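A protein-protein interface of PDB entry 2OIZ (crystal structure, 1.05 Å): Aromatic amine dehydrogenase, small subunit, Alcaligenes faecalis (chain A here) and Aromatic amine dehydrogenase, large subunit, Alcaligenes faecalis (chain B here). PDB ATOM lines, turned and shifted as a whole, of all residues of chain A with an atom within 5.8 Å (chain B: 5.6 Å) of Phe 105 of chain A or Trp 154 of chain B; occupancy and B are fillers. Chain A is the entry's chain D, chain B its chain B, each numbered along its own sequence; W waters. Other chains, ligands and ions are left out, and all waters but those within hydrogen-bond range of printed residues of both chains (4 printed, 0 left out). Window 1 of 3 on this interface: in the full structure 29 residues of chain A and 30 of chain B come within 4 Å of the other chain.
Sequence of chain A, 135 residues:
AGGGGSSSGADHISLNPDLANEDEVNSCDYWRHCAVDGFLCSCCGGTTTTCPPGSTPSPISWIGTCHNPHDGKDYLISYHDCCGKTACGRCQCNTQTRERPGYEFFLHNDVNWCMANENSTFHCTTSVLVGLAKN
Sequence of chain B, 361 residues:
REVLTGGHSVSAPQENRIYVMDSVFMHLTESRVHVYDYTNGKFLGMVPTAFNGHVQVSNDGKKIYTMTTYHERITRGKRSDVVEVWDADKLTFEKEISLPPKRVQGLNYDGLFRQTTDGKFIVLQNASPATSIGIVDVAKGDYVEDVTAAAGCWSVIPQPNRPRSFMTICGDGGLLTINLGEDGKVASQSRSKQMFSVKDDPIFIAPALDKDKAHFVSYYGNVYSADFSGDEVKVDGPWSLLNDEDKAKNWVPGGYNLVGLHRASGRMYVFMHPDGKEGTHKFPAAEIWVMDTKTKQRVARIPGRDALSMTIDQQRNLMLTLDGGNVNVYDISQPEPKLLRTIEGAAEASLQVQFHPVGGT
Of the 18 printed residues of chain B, 5 touch a printed residue of chain A. Hydrophobic or aromatic side chains of chain B that line the printed part of chain A: Ala 127, Pro 129, Trp 154, Ile 169 and Ile 205. Along chain B the printed residues that touch a printed residue of chain A span positions 127 to 205. Hydrophobic or aromatic side chains of chain A within 4 Å of the printed part of chain B: Pro 101, Tyr 103, Phe 105, Val 111, Trp 113 and Met 115.
The backbone carbonyl oxygen (O) of Ala 127 of chain B sits close to the side-chain sulfur (SD) of Met 115 of chain A, 3.6 Å away.
Water W2 lies within hydrogen-bond range of O of Tyr 103 of chain A (2.7 Å) and O of Gly 152 of chain B (2.7 Å). Water W4 bridges NE2 of His 108 of chain A (2.7 Å) and NE1 of Trp 154 of chain B (2.8 Å). Water W1 lies within hydrogen-bond range of O of Gly 102 of chain A (2.8 Å) and O of Cys 153 of chain B (2.9 Å). Water W3 lies within hydrogen-bond range of the backbone NH of Gly 102 of chain A (2.9 Å), the indole nitrogen of Trp 154 of chain B (3.4 Å) and a ring nitrogen (NE2) of His 108 of chain A (3.5 Å).
Phe 105 of chain A touches just these residues of chain B: Ala 127 (3.8 Å), Pro 129 (3.6 Å) and Trp 154 (3.3 Å). Of chain A, only Gly 102 (3.5 Å), Tyr 103 (3.5 Å), Phe 105 (3.3 Å) and Val 111 (3.9 Å) come within 4 Å of Trp 154 of chain B. Of the printed residues of chain B, Pro 101 of chain A touches Ile 205. Of the printed residues of chain B, Val 111 of chain A touches Trp 154 (3.9 Å). Of the printed residues of chain B, Tyr 103 of chain A touches Trp 154 (3.5 Å), Ile 169 (3.6 Å) and Ile 205 (3.9 Å). Of the printed residues of chain B, Gly 102 of chain A touches Trp 154. Of the printed residues of chain A, Ile 205 of chain B touches Pro 101 (3.8 Å) and Tyr 103 (3.9 Å). The nearest printed residue of chain B that does not touch Pro 101 of chain A is Trp 154 of chain B (5.1 Å).
CD1 of Trp 113 of chain A is covalently linked to CE3 of TRQ 62 of chain A (1.5 Å). NE1 of Trp 113 of chain A lies within hydrogen-bond range of O of His 108 of chain A (3.0 Å). The side-chain hydroxyl of Thr 168 of chain B sits close to the backbone carbonyl oxygen of Trp 154 of chain B (3.3 Å). The backbone carbonyl oxygen of Ile 169 of chain B sits at hydrogen-bond distance from the backbone NH of Trp 154 of chain B (2.8 Å). SG of Cys 170 of chain B is disulfide-bonded to SG of Cys 153 of chain B, 2.0 Å away.
Pro 101 of chain A touches Ile 205 of chain B (CB to CG2, 3.8 Å). CB of Trp 154 of chain B touches C of Gly 102 of chain A (3.5 Å). Trp 154 of chain B touches Tyr 103 of chain A (CB to N, 3.5 Å). Ile 205 of chain B touches Tyr 103 of chain A (CG2 to CE2, 3.9 Å). CZ of Phe 105 of chain A touches CB of Ala 127 of chain B, 3.8 Å away. Pro 129 of chain B touches Phe 105 of chain A. Trp 154 of chain B touches Phe 105 of chain A (CH2 to CE1, 3.3 Å). Val 111 of chain A touches Trp 154 of chain B (CG1 to CZ2, 3.9 Å). CB of Pro 129 of chain B touches CZ3 of Trp 113 of chain A, 3.8 Å away. Met 115 of chain A touches Pro 129 of chain B.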
ATOM      1  N   TRQ A  62     -17.508 -24.364  30.392  1.00  0.00           N
ATOM      2  CA  TRQ A  62     -17.767 -23.042  30.916  1.00  0.00           C
ATOM      3  C   TRQ A  62     -17.970 -23.148  32.430  1.00  0.00           C
ATOM      4  O   TRQ A  62     -18.096 -24.246  32.982  1.00  0.00           O
ATOM      5  CB  TRQ A  62     -18.949 -22.386  30.186  1.00  0.00           C
ATOM      6  CG  TRQ A  62     -20.288 -23.079  30.249  1.00  0.00           C
ATOM      7  CD1 TRQ A  62     -21.225 -22.808  31.183  1.00  0.00           C
ATOM      8  NE1 TRQ A  62     -22.367 -23.506  30.957  1.00  0.00           N
ATOM      9  CE2 TRQ A  62     -22.207 -24.277  29.841  1.00  0.00           C
ATOM     10  CZ2 TRQ A  62     -23.120 -25.134  29.238  1.00  0.00           C
ATOM     11  CH2 TRQ A  62     -22.728 -25.788  28.110  1.00  0.00           C
ATOM     12  CZ3 TRQ A  62     -21.446 -25.593  27.575  1.00  0.00           C
ATOM     13  CE3 TRQ A  62     -20.523 -24.726  28.185  1.00  0.00           C
ATOM     14  CD2 TRQ A  62     -20.913 -24.047  29.342  1.00  0.00           C
ATOM     15  O7  TRQ A  62     -24.316 -25.214  29.916  1.00  0.00           O
ATOM     16  N   PRO A 101     -20.507 -13.265  26.485  1.00  0.00           N
ATOM     17  CA  PRO A 101     -20.319 -13.759  25.123  1.00  0.00           C
ATOM     18  C   PRO A 101     -18.944 -14.397  24.911  1.00  0.00           C
ATOM     19  O   PRO A 101     -18.083 -14.435  25.796  1.00  0.00           O
ATOM     20  CB  PRO A 101     -20.480 -12.509  24.256  1.00  0.00           C
ATOM     21  CG  PRO A 101     -21.257 -11.527  25.144  1.00  0.00           C
ATOM     22  CD  PRO A 101     -20.697 -11.800  26.514  1.00  0.00           C
ATOM     23  N   GLY A 102     -18.726 -14.837  23.662  1.00  0.00           N
ATOM     24  CA  GLY A 102     -17.573 -15.670  23.371  1.00  0.00           C
ATOM     25  C   GLY A 102     -16.224 -14.978  23.447  1.00  0.00           C
ATOM     26  O   GLY A 102     -15.199 -15.659  23.477  1.00  0.00           O
ATOM     27  N   TYR A 103     -16.193 -13.634  23.515  1.00  0.00           N
ATOM     28  CA  TYR A 103     -14.968 -12.909  23.813  1.00  0.00           C
ATOM     29  C   TYR A 103     -14.554 -13.023  25.287  1.00  0.00           C
ATOM     30  O   TYR A 103     -13.460 -12.596  25.644  1.00  0.00           O
ATOM     31  CB  TYR A 103     -15.030 -11.465  23.290  1.00  0.00           C
ATOM     32  CG  TYR A 103     -16.159 -10.657  23.877  1.00  0.00           C
ATOM     33  CD1 TYR A 103     -16.119 -10.217  25.192  1.00  0.00           C
ATOM     34  CD2 TYR A 103     -17.278 -10.361  23.125  1.00  0.00           C
ATOM     35  CE1 TYR A 103     -17.180  -9.472  25.730  1.00  0.00           C
ATOM     36  CE2 TYR A 103     -18.343  -9.631  23.661  1.00  0.00           C
ATOM     37  CZ  TYR A 103     -18.284  -9.204  24.967  1.00  0.00           C
ATOM     38  OH  TYR A 103     -19.297  -8.462  25.534  1.00  0.00           O
ATOM     39  N   GLU A 104     -15.399 -13.602  26.164  1.00  0.00           N
ATOM     40  CA  GLU A 104     -15.021 -14.108  27.505  1.00  0.00           C
ATOM     41  C   GLU A 104     -15.358 -15.599  27.524  1.00  0.00           C
ATOM     42  O   GLU A 104     -16.343 -16.040  28.141  1.00  0.00           O
ATOM     43  CB  GLU A 104     -15.823 -13.372  28.583  1.00  0.00           C
ATOM     44  CG  GLU A 104     -15.758 -11.848  28.536  1.00  0.00           C
ATOM     45  CD  GLU A 104     -16.617 -11.180  29.623  1.00  0.00           C
ATOM     46  OE1 GLU A 104     -16.355 -11.503  30.785  1.00  0.00           O
ATOM     47  OE2 GLU A 104     -17.542 -10.341  29.345  1.00  0.00           O
ATOM     48  N   PHE A 105     -14.546 -16.369  26.807  1.00  0.00           N
ATOM     49  CA  PHE A 105     -15.003 -17.654  26.291  1.00  0.00           C
ATOM     50  C   PHE A 105     -15.395 -18.627  27.400  1.00  0.00           C
ATOM     51  O   PHE A 105     -16.376 -19.362  27.209  1.00  0.00           O
ATOM     52  CB  PHE A 105     -13.941 -18.250  25.360  1.00  0.00           C
ATOM     53  CG  PHE A 105     -14.466 -19.294  24.406  1.00  0.00           C
ATOM     54  CD1 PHE A 105     -15.521 -19.037  23.581  1.00  0.00           C
ATOM     55  CD2 PHE A 105     -13.901 -20.556  24.344  1.00  0.00           C
ATOM     56  CE1 PHE A 105     -15.974 -19.985  22.678  1.00  0.00           C
ATOM     57  CE2 PHE A 105     -14.381 -21.511  23.468  1.00  0.00           C
ATOM     58  CZ  PHE A 105     -15.410 -21.216  22.628  1.00  0.00           C
ATOM     59  N   PHE A 106     -14.652 -18.676  28.499  1.00  0.00           N
ATOM     60  CA  PHE A 106     -14.964 -19.672  29.505  1.00  0.00           C
ATOM     61  C   PHE A 106     -16.113 -19.276  30.408  1.00  0.00           C
ATOM     62  O   PHE A 106     -16.460 -20.065  31.275  1.00  0.00           O
ATOM     63  CB  PHE A 106     -13.727 -20.138  30.250  1.00  0.00           C
ATOM     64  CG  PHE A 106     -12.757 -20.809  29.338  1.00  0.00           C
ATOM     65  CD1 PHE A 106     -11.773 -20.069  28.692  1.00  0.00           C
ATOM     66  CD2 PHE A 106     -12.873 -22.159  29.045  1.00  0.00           C
ATOM     67  CE1 PHE A 106     -10.889 -20.674  27.807  1.00  0.00           C
ATOM     68  CE2 PHE A 106     -11.967 -22.788  28.170  1.00  0.00           C
ATOM     69  CZ  PHE A 106     -10.991 -22.033  27.540  1.00  0.00           C
ATOM     70  N   LEU A 107     -16.740 -18.122  30.142  1.00  0.00           N
ATOM     71  CA  LEU A 107     -17.992 -17.764  30.782  1.00  0.00           C
ATOM     72  C   LEU A 107     -19.186 -17.943  29.856  1.00  0.00           C
ATOM     73  O   LEU A 107     -20.291 -17.543  30.226  1.00  0.00           O
ATOM     74  CB  LEU A 107     -17.966 -16.302  31.259  1.00  0.00           C
ATOM     75  CG  LEU A 107     -16.898 -15.971  32.288  1.00  0.00           C
ATOM     76  CD1 LEU A 107     -16.990 -14.486  32.630  1.00  0.00           C
ATOM     77  CD2 LEU A 107     -17.023 -16.792  33.549  1.00  0.00           C
ATOM     78  N   HIS A 108     -18.986 -18.518  28.672  1.00  0.00           N
ATOM     79  CA  HIS A 108     -19.960 -18.466  27.608  1.00  0.00           C
ATOM     80  C   HIS A 108     -20.634 -19.834  27.416  1.00  0.00           C
ATOM     81  O   HIS A 108     -19.941 -20.857  27.346  1.00  0.00           O
ATOM     82  CB  HIS A 108     -19.215 -18.062  26.322  1.00  0.00           C
ATOM     83  CG  HIS A 108     -20.097 -17.950  25.108  1.00  0.00           C
ATOM     84  ND1 HIS A 108     -21.273 -17.230  25.082  1.00  0.00           N
ATOM     85  CD2 HIS A 108     -19.948 -18.452  23.842  1.00  0.00           C
ATOM     86  CE1 HIS A 108     -21.806 -17.320  23.869  1.00  0.00           C
ATOM     87  NE2 HIS A 108     -21.023 -18.063  23.095  1.00  0.00           N
ATOM     88  N   ASN A 109     -21.963 -19.860  27.286  1.00  0.00           N
ATOM     89  CA  ASN A 109     -22.692 -21.131  27.263  1.00  0.00           C
ATOM     90  C   ASN A 109     -23.511 -21.362  26.003  1.00  0.00           C
ATOM     91  O   ASN A 109     -24.348 -22.264  25.981  1.00  0.00           O
ATOM     92  CB  ASN A 109     -23.540 -21.348  28.538  1.00  0.00           C
ATOM     93  CG  ASN A 109     -24.786 -20.504  28.610  1.00  0.00           C
ATOM     94  OD1 ASN A 109     -25.186 -19.852  27.646  1.00  0.00           O
ATOM     95  ND2 ASN A 109     -25.442 -20.550  29.788  1.00  0.00           N
ATOM     96  N   VAL A 111     -21.929 -22.318  23.237  1.00  0.00           N
ATOM     97  CA  VAL A 111     -21.082 -23.230  22.510  1.00  0.00           C
ATOM     98  C   VAL A 111     -21.176 -24.594  23.133  1.00  0.00           C
ATOM     99  O   VAL A 111     -21.615 -24.755  24.271  1.00  0.00           O
ATOM    100  CB  VAL A 111     -19.633 -22.732  22.459  1.00  0.00           C
ATOM    101  CG1 VAL A 111     -19.513 -21.483  21.558  1.00  0.00           C
ATOM    102  CG2 VAL A 111     -19.077 -22.493  23.862  1.00  0.00           C
ATOM    103  N   TRP A 113     -19.583 -27.410  24.882  1.00  0.00           N
ATOM    104  CA  TRP A 113     -18.390 -27.678  25.671  1.00  0.00           C
ATOM    105  C   TRP A 113     -17.874 -29.119  25.494  1.00  0.00           C
ATOM    106  O   TRP A 113     -16.832 -29.452  26.041  1.00  0.00           O
ATOM    107  CB  TRP A 113     -18.534 -27.186  27.141  1.00  0.00           C
ATOM    108  CG  TRP A 113     -18.285 -25.674  27.218  1.00  0.00           C
ATOM    109  CD1 TRP A 113     -19.142 -24.661  27.594  1.00  0.00           C
ATOM    110  CD2 TRP A 113     -17.075 -25.028  26.839  1.00  0.00           C
ATOM    111  NE1 TRP A 113     -18.534 -23.450  27.471  1.00  0.00           N
ATOM    112  CE2 TRP A 113     -17.260 -23.643  27.004  1.00  0.00           C
ATOM    113  CE3 TRP A 113     -15.847 -25.493  26.382  1.00  0.00           C
ATOM    114  CZ2 TRP A 113     -16.258 -22.722  26.730  1.00  0.00           C
ATOM    115  CZ3 TRP A 113     -14.855 -24.579  26.113  1.00  0.00           C
ATOM    116  CH2 TRP A 113     -15.064 -23.212  26.286  1.00  0.00           C
ATOM    117  N   MET A 115     -16.804 -29.780  22.522  1.00  0.00           N
ATOM    118  CA  MET A 115     -16.115 -29.505  21.259  1.00  0.00           C
ATOM    119  C   MET A 115     -14.759 -30.166  21.083  1.00  0.00           C
ATOM    120  O   MET A 115     -14.299 -30.299  19.941  1.00  0.00           O
ATOM    121  CB  MET A 115     -15.971 -27.975  21.055  1.00  0.00           C
ATOM    122  CG  MET A 115     -15.021 -27.316  22.016  1.00  0.00           C
ATOM    123  SD  MET A 115     -14.935 -25.512  21.865  1.00  0.00           S
ATOM    124  CE  MET A 115     -16.232 -24.985  22.964  1.00  0.00           C
ATOM    125  N   VAL B 104     -16.354 -23.973  14.974  1.00  0.00           N
ATOM    126  CA  VAL B 104     -17.210 -23.687  16.131  1.00  0.00           C
ATOM    127  C   VAL B 104     -18.474 -24.526  16.110  1.00  0.00           C
ATOM    128  O   VAL B 104     -19.198 -24.522  15.108  1.00  0.00           O
ATOM    129  CB  VAL B 104     -17.573 -22.211  16.262  1.00  0.00           C
ATOM    130  CG1 VAL B 104     -18.322 -21.664  15.034  1.00  0.00           C
ATOM    131  CG2 VAL B 104     -18.358 -21.964  17.537  1.00  0.00           C
ATOM    132  N   LEU B 112     -20.477 -16.248  13.203  1.00  0.00           N
ATOM    133  CA  LEU B 112     -19.658 -17.445  13.273  1.00  0.00           C
ATOM    134  C   LEU B 112     -19.310 -18.026  11.903  1.00  0.00           C
ATOM    135  O   LEU B 112     -18.433 -18.880  11.798  1.00  0.00           O
ATOM    136  CB  LEU B 112     -20.333 -18.473  14.188  1.00  0.00           C
ATOM    137  CG  LEU B 112     -20.505 -17.950  15.629  1.00  0.00           C
ATOM    138  CD1 LEU B 112     -21.228 -18.993  16.500  1.00  0.00           C
ATOM    139  CD2 LEU B 112     -19.215 -17.547  16.257  1.00  0.00           C
ATOM    140  N   GLN B 125     -15.449 -19.056  12.427  1.00  0.00           N
ATOM    141  CA  GLN B 125     -14.880 -19.116  13.749  1.00  0.00           C
ATOM    142  C   GLN B 125     -14.482 -20.552  14.108  1.00  0.00           C
ATOM    143  O   GLN B 125     -15.299 -21.456  13.982  1.00  0.00           O
ATOM    144  CB  GLN B 125     -15.905 -18.562  14.737  1.00  0.00           C
ATOM    145  CG  GLN B 125     -15.417 -18.468  16.144  1.00  0.00           C
ATOM    146  CD  GLN B 125     -14.250 -17.508  16.351  1.00  0.00           C
ATOM    147  OE1 GLN B 125     -13.123 -17.950  16.660  1.00  0.00           O
ATOM    148  NE2 GLN B 125     -14.466 -16.263  16.098  1.00  0.00           N
ATOM    149  N   ASN B 126     -13.253 -20.697  14.598  1.00  0.00           N
ATOM    150  CA  ASN B 126     -12.769 -21.942  15.142  1.00  0.00           C
ATOM    151  C   ASN B 126     -12.695 -21.850  16.680  1.00  0.00           C
ATOM    152  O   ASN B 126     -12.463 -20.773  17.250  1.00  0.00           O
ATOM    153  CB  ASN B 126     -11.343 -22.248  14.690  1.00  0.00           C
ATOM    154  CG  ASN B 126     -11.227 -22.584  13.249  1.00  0.00           C
ATOM    155  OD1 ASN B 126     -12.088 -23.263  12.702  1.00  0.00           O
ATOM    156  ND2 ASN B 126     -10.093 -22.157  12.626  1.00  0.00           N
ATOM    157  N   ALA B 127     -12.826 -22.996  17.326  1.00  0.00           N
ATOM    158  CA  ALA B 127     -12.609 -23.084  18.777  1.00  0.00           C
ATOM    159  C   ALA B 127     -12.215 -24.506  19.101  1.00  0.00           C
ATOM    160  O   ALA B 127     -12.966 -25.453  18.839  1.00  0.00           O
ATOM    161  CB  ALA B 127     -13.846 -22.726  19.556  1.00  0.00           C
ATOM    162  N   PRO B 129     -10.488 -25.586  22.488  1.00  0.00           N
ATOM    163  CA  PRO B 129     -11.251 -24.354  22.581  1.00  0.00           C
ATOM    164  C   PRO B 129     -10.448 -23.075  22.322  1.00  0.00           C
ATOM    165  O   PRO B 129     -11.046 -22.013  22.301  1.00  0.00           O
ATOM    166  CB  PRO B 129     -11.708 -24.357  24.041  1.00  0.00           C
ATOM    167  CG  PRO B 129     -10.593 -25.026  24.771  1.00  0.00           C
ATOM    168  CD  PRO B 129     -10.157 -26.116  23.836  1.00  0.00           C
ATOM    169  N   THR B 131      -9.212 -20.093  20.290  1.00  0.00           N
ATOM    170  CA  THR B 131      -9.940 -19.495  19.189  1.00  0.00           C
ATOM    171  C   THR B 131      -9.000 -19.013  18.088  1.00  0.00           C
ATOM    172  O   THR B 131      -7.879 -18.560  18.320  1.00  0.00           O
ATOM    173  CB  THR B 131     -10.944 -18.389  19.615  1.00  0.00           C
ATOM    174  OG1 THR B 131     -10.287 -17.165  19.887  1.00  0.00           O
ATOM    175  CG2 THR B 131     -11.764 -18.854  20.774  1.00  0.00           C
ATOM    176  N   ALA B 150      -6.173 -13.793  15.922  1.00  0.00           N
ATOM    177  CA  ALA B 150      -7.499 -13.653  16.535  1.00  0.00           C
ATOM    178  C   ALA B 150      -7.694 -14.484  17.814  1.00  0.00           C
ATOM    179  O   ALA B 150      -8.799 -14.514  18.353  1.00  0.00           O
ATOM    180  CB  ALA B 150      -8.571 -13.976  15.499  1.00  0.00           C
ATOM    181  N   GLY B 152      -8.293 -15.327  21.455  1.00  0.00           N
ATOM    182  CA  GLY B 152      -8.910 -14.531  22.507  1.00  0.00           C
ATOM    183  C   GLY B 152      -9.964 -13.564  21.991  1.00  0.00           C
ATOM    184  O   GLY B 152     -10.448 -12.712  22.735  1.00  0.00           O
ATOM    185  N   CYS B 153     -10.273 -13.669  20.710  1.00  0.00           N
ATOM    186  CA  CYS B 153     -11.304 -12.872  20.074  1.00  0.00           C
ATOM    187  C   CYS B 153     -12.487 -13.780  19.676  1.00  0.00           C
ATOM    188  O   CYS B 153     -12.412 -15.025  19.818  1.00  0.00           O
ATOM    189  CB  CYS B 153     -10.776 -12.126  18.845  1.00  0.00           C
ATOM    190  SG  CYS B 153      -9.278 -11.176  19.145  1.00  0.00           S
ATOM    191  N   TRP B 154     -13.574 -13.190  19.185  1.00  0.00           N
ATOM    192  CA  TRP B 154     -14.748 -13.981  18.862  1.00  0.00           C
ATOM    193  C   TRP B 154     -15.579 -13.252  17.825  1.00  0.00           C
ATOM    194  O   TRP B 154     -15.938 -12.072  17.976  1.00  0.00           O
ATOM    195  CB  TRP B 154     -15.602 -14.240  20.100  1.00  0.00           C
ATOM    196  CG  TRP B 154     -16.626 -15.307  19.934  1.00  0.00           C
ATOM    197  CD1 TRP B 154     -17.992 -15.178  19.948  1.00  0.00           C
ATOM    198  CD2 TRP B 154     -16.359 -16.691  19.754  1.00  0.00           C
ATOM    199  NE1 TRP B 154     -18.583 -16.410  19.789  1.00  0.00           N
ATOM    200  CE2 TRP B 154     -17.599 -17.359  19.676  1.00  0.00           C
ATOM    201  CE3 TRP B 154     -15.183 -17.436  19.679  1.00  0.00           C
ATOM    202  CZ2 TRP B 154     -17.682 -18.730  19.502  1.00  0.00           C
ATOM    203  CZ3 TRP B 154     -15.265 -18.794  19.512  1.00  0.00           C
ATOM    204  CH2 TRP B 154     -16.507 -19.433  19.428  1.00  0.00           C
ATOM    205  N   SER B 155     -15.946 -14.015  16.796  1.00  0.00           N
ATOM    206  CA  SER B 155     -16.896 -13.682  15.744  1.00  0.00           C
ATOM    207  C   SER B 155     -16.298 -12.799  14.629  1.00  0.00           C
ATOM    208  O   SER B 155     -15.269 -12.159  14.812  1.00  0.00           O
ATOM    209  CB  SER B 155     -18.219 -13.117  16.274  1.00  0.00           C
ATOM    210  OG  SER B 155     -18.171 -11.734  16.494  1.00  0.00           O
ATOM    211  N   VAL B 156     -16.984 -12.763  13.494  1.00  0.00           N
ATOM    212  CA  VAL B 156     -16.473 -12.166  12.274  1.00  0.00           C
ATOM    213  C   VAL B 156     -17.476 -11.093  11.810  1.00  0.00           C
ATOM    214  O   VAL B 156     -18.655 -11.407  11.558  1.00  0.00           O
ATOM    215  CB  VAL B 156     -16.329 -13.227  11.155  1.00  0.00           C
ATOM    216  CG1 VAL B 156     -15.880 -12.599   9.859  1.00  0.00           C
ATOM    217  CG2 VAL B 156     -15.405 -14.346  11.588  1.00  0.00           C
ATOM    218  N   ILE B 157     -16.989  -9.862  11.667  1.00  0.00           N
ATOM    219  CA  ILE B 157     -17.786  -8.739  11.141  1.00  0.00           C
ATOM    220  C   ILE B 157     -17.108  -8.272   9.865  1.00  0.00           C
ATOM    221  O   ILE B 157     -16.086  -7.601   9.895  1.00  0.00           O
ATOM    222  CB  ILE B 157     -17.860  -7.585  12.147  1.00  0.00           C
ATOM    223  CG1 ILE B 157     -18.426  -8.055  13.509  1.00  0.00           C
ATOM    224  CG2 ILE B 157     -18.751  -6.495  11.592  1.00  0.00           C
ATOM    225  CD1 ILE B 157     -17.473  -8.125  14.628  1.00  0.00           C
ATOM    226  N   THR B 168     -12.954  -8.599  14.306  1.00  0.00           N
ATOM    227  CA  THR B 168     -13.403  -9.507  15.347  1.00  0.00           C
ATOM    228  C   THR B 168     -13.345  -8.774  16.696  1.00  0.00           C
ATOM    229  O   THR B 168     -12.596  -7.816  16.863  1.00  0.00           O
ATOM    230  CB  THR B 168     -12.613 -10.833  15.336  1.00  0.00           C
ATOM    231  OG1 THR B 168     -13.162 -11.723  16.298  1.00  0.00           O
ATOM    232  CG2 THR B 168     -11.153 -10.608  15.593  1.00  0.00           C
ATOM    233  N   ILE B 169     -14.187  -9.190  17.622  1.00  0.00           N
ATOM    234  CA  ILE B 169     -14.266  -8.571  18.939  1.00  0.00           C
ATOM    235  C   ILE B 169     -13.329  -9.283  19.895  1.00  0.00           C
ATOM    236  O   ILE B 169     -13.393 -10.505  20.026  1.00  0.00           O
ATOM    237  CB  ILE B 169     -15.701  -8.645  19.486  1.00  0.00           C
ATOM    238  CG1 ILE B 169     -16.709  -8.012  18.530  1.00  0.00           C
ATOM    239  CG2 ILE B 169     -15.747  -8.015  20.861  1.00  0.00           C
ATOM    240  CD1 ILE B 169     -18.151  -8.385  18.823  1.00  0.00           C
ATOM    241  N   CYS B 170     -12.426  -8.548  20.515  1.00  0.00           N
ATOM    242  CA  CYS B 170     -11.433  -9.175  21.389  1.00  0.00           C
ATOM    243  C   CYS B 170     -11.726  -9.013  22.863  1.00  0.00           C
ATOM    244  O   CYS B 170     -12.472  -8.152  23.300  1.00  0.00           O
ATOM    245  CB  CYS B 170     -10.039  -8.764  21.004  1.00  0.00           C
ATOM    246  SG  CYS B 170      -9.743  -9.203  19.261  1.00  0.00           S
ATOM    247  N   ILE B 205     -22.558  -9.561  20.672  1.00  0.00           N
ATOM    248  CA  ILE B 205     -21.648  -9.656  19.524  1.00  0.00           C
ATOM    249  C   ILE B 205     -22.316  -9.250  18.210  1.00  0.00           C
ATOM    250  O   ILE B 205     -21.631  -8.902  17.240  1.00  0.00           O
ATOM    251  CB  ILE B 205     -21.005 -11.067  19.390  1.00  0.00           C
ATOM    252  CG1 ILE B 205     -22.050 -12.165  19.080  1.00  0.00           C
ATOM    253  CG2 ILE B 205     -20.160 -11.365  20.624  1.00  0.00           C
ATOM    254  CD1 ILE B 205     -21.426 -13.431  18.565  1.00  0.00           C
HETATM  255  O   HOH W   1     -12.541 -15.769  22.609  1.00  0.00           O
HETATM  256  O   HOH W   2     -10.857 -13.251  25.367  1.00  0.00           O
HETATM  257  O   HOH W   3     -20.953 -14.865  21.749  1.00  0.00           O
HETATM  258  O   HOH W   4     -21.139 -17.450  20.422  1.00  0.00           O
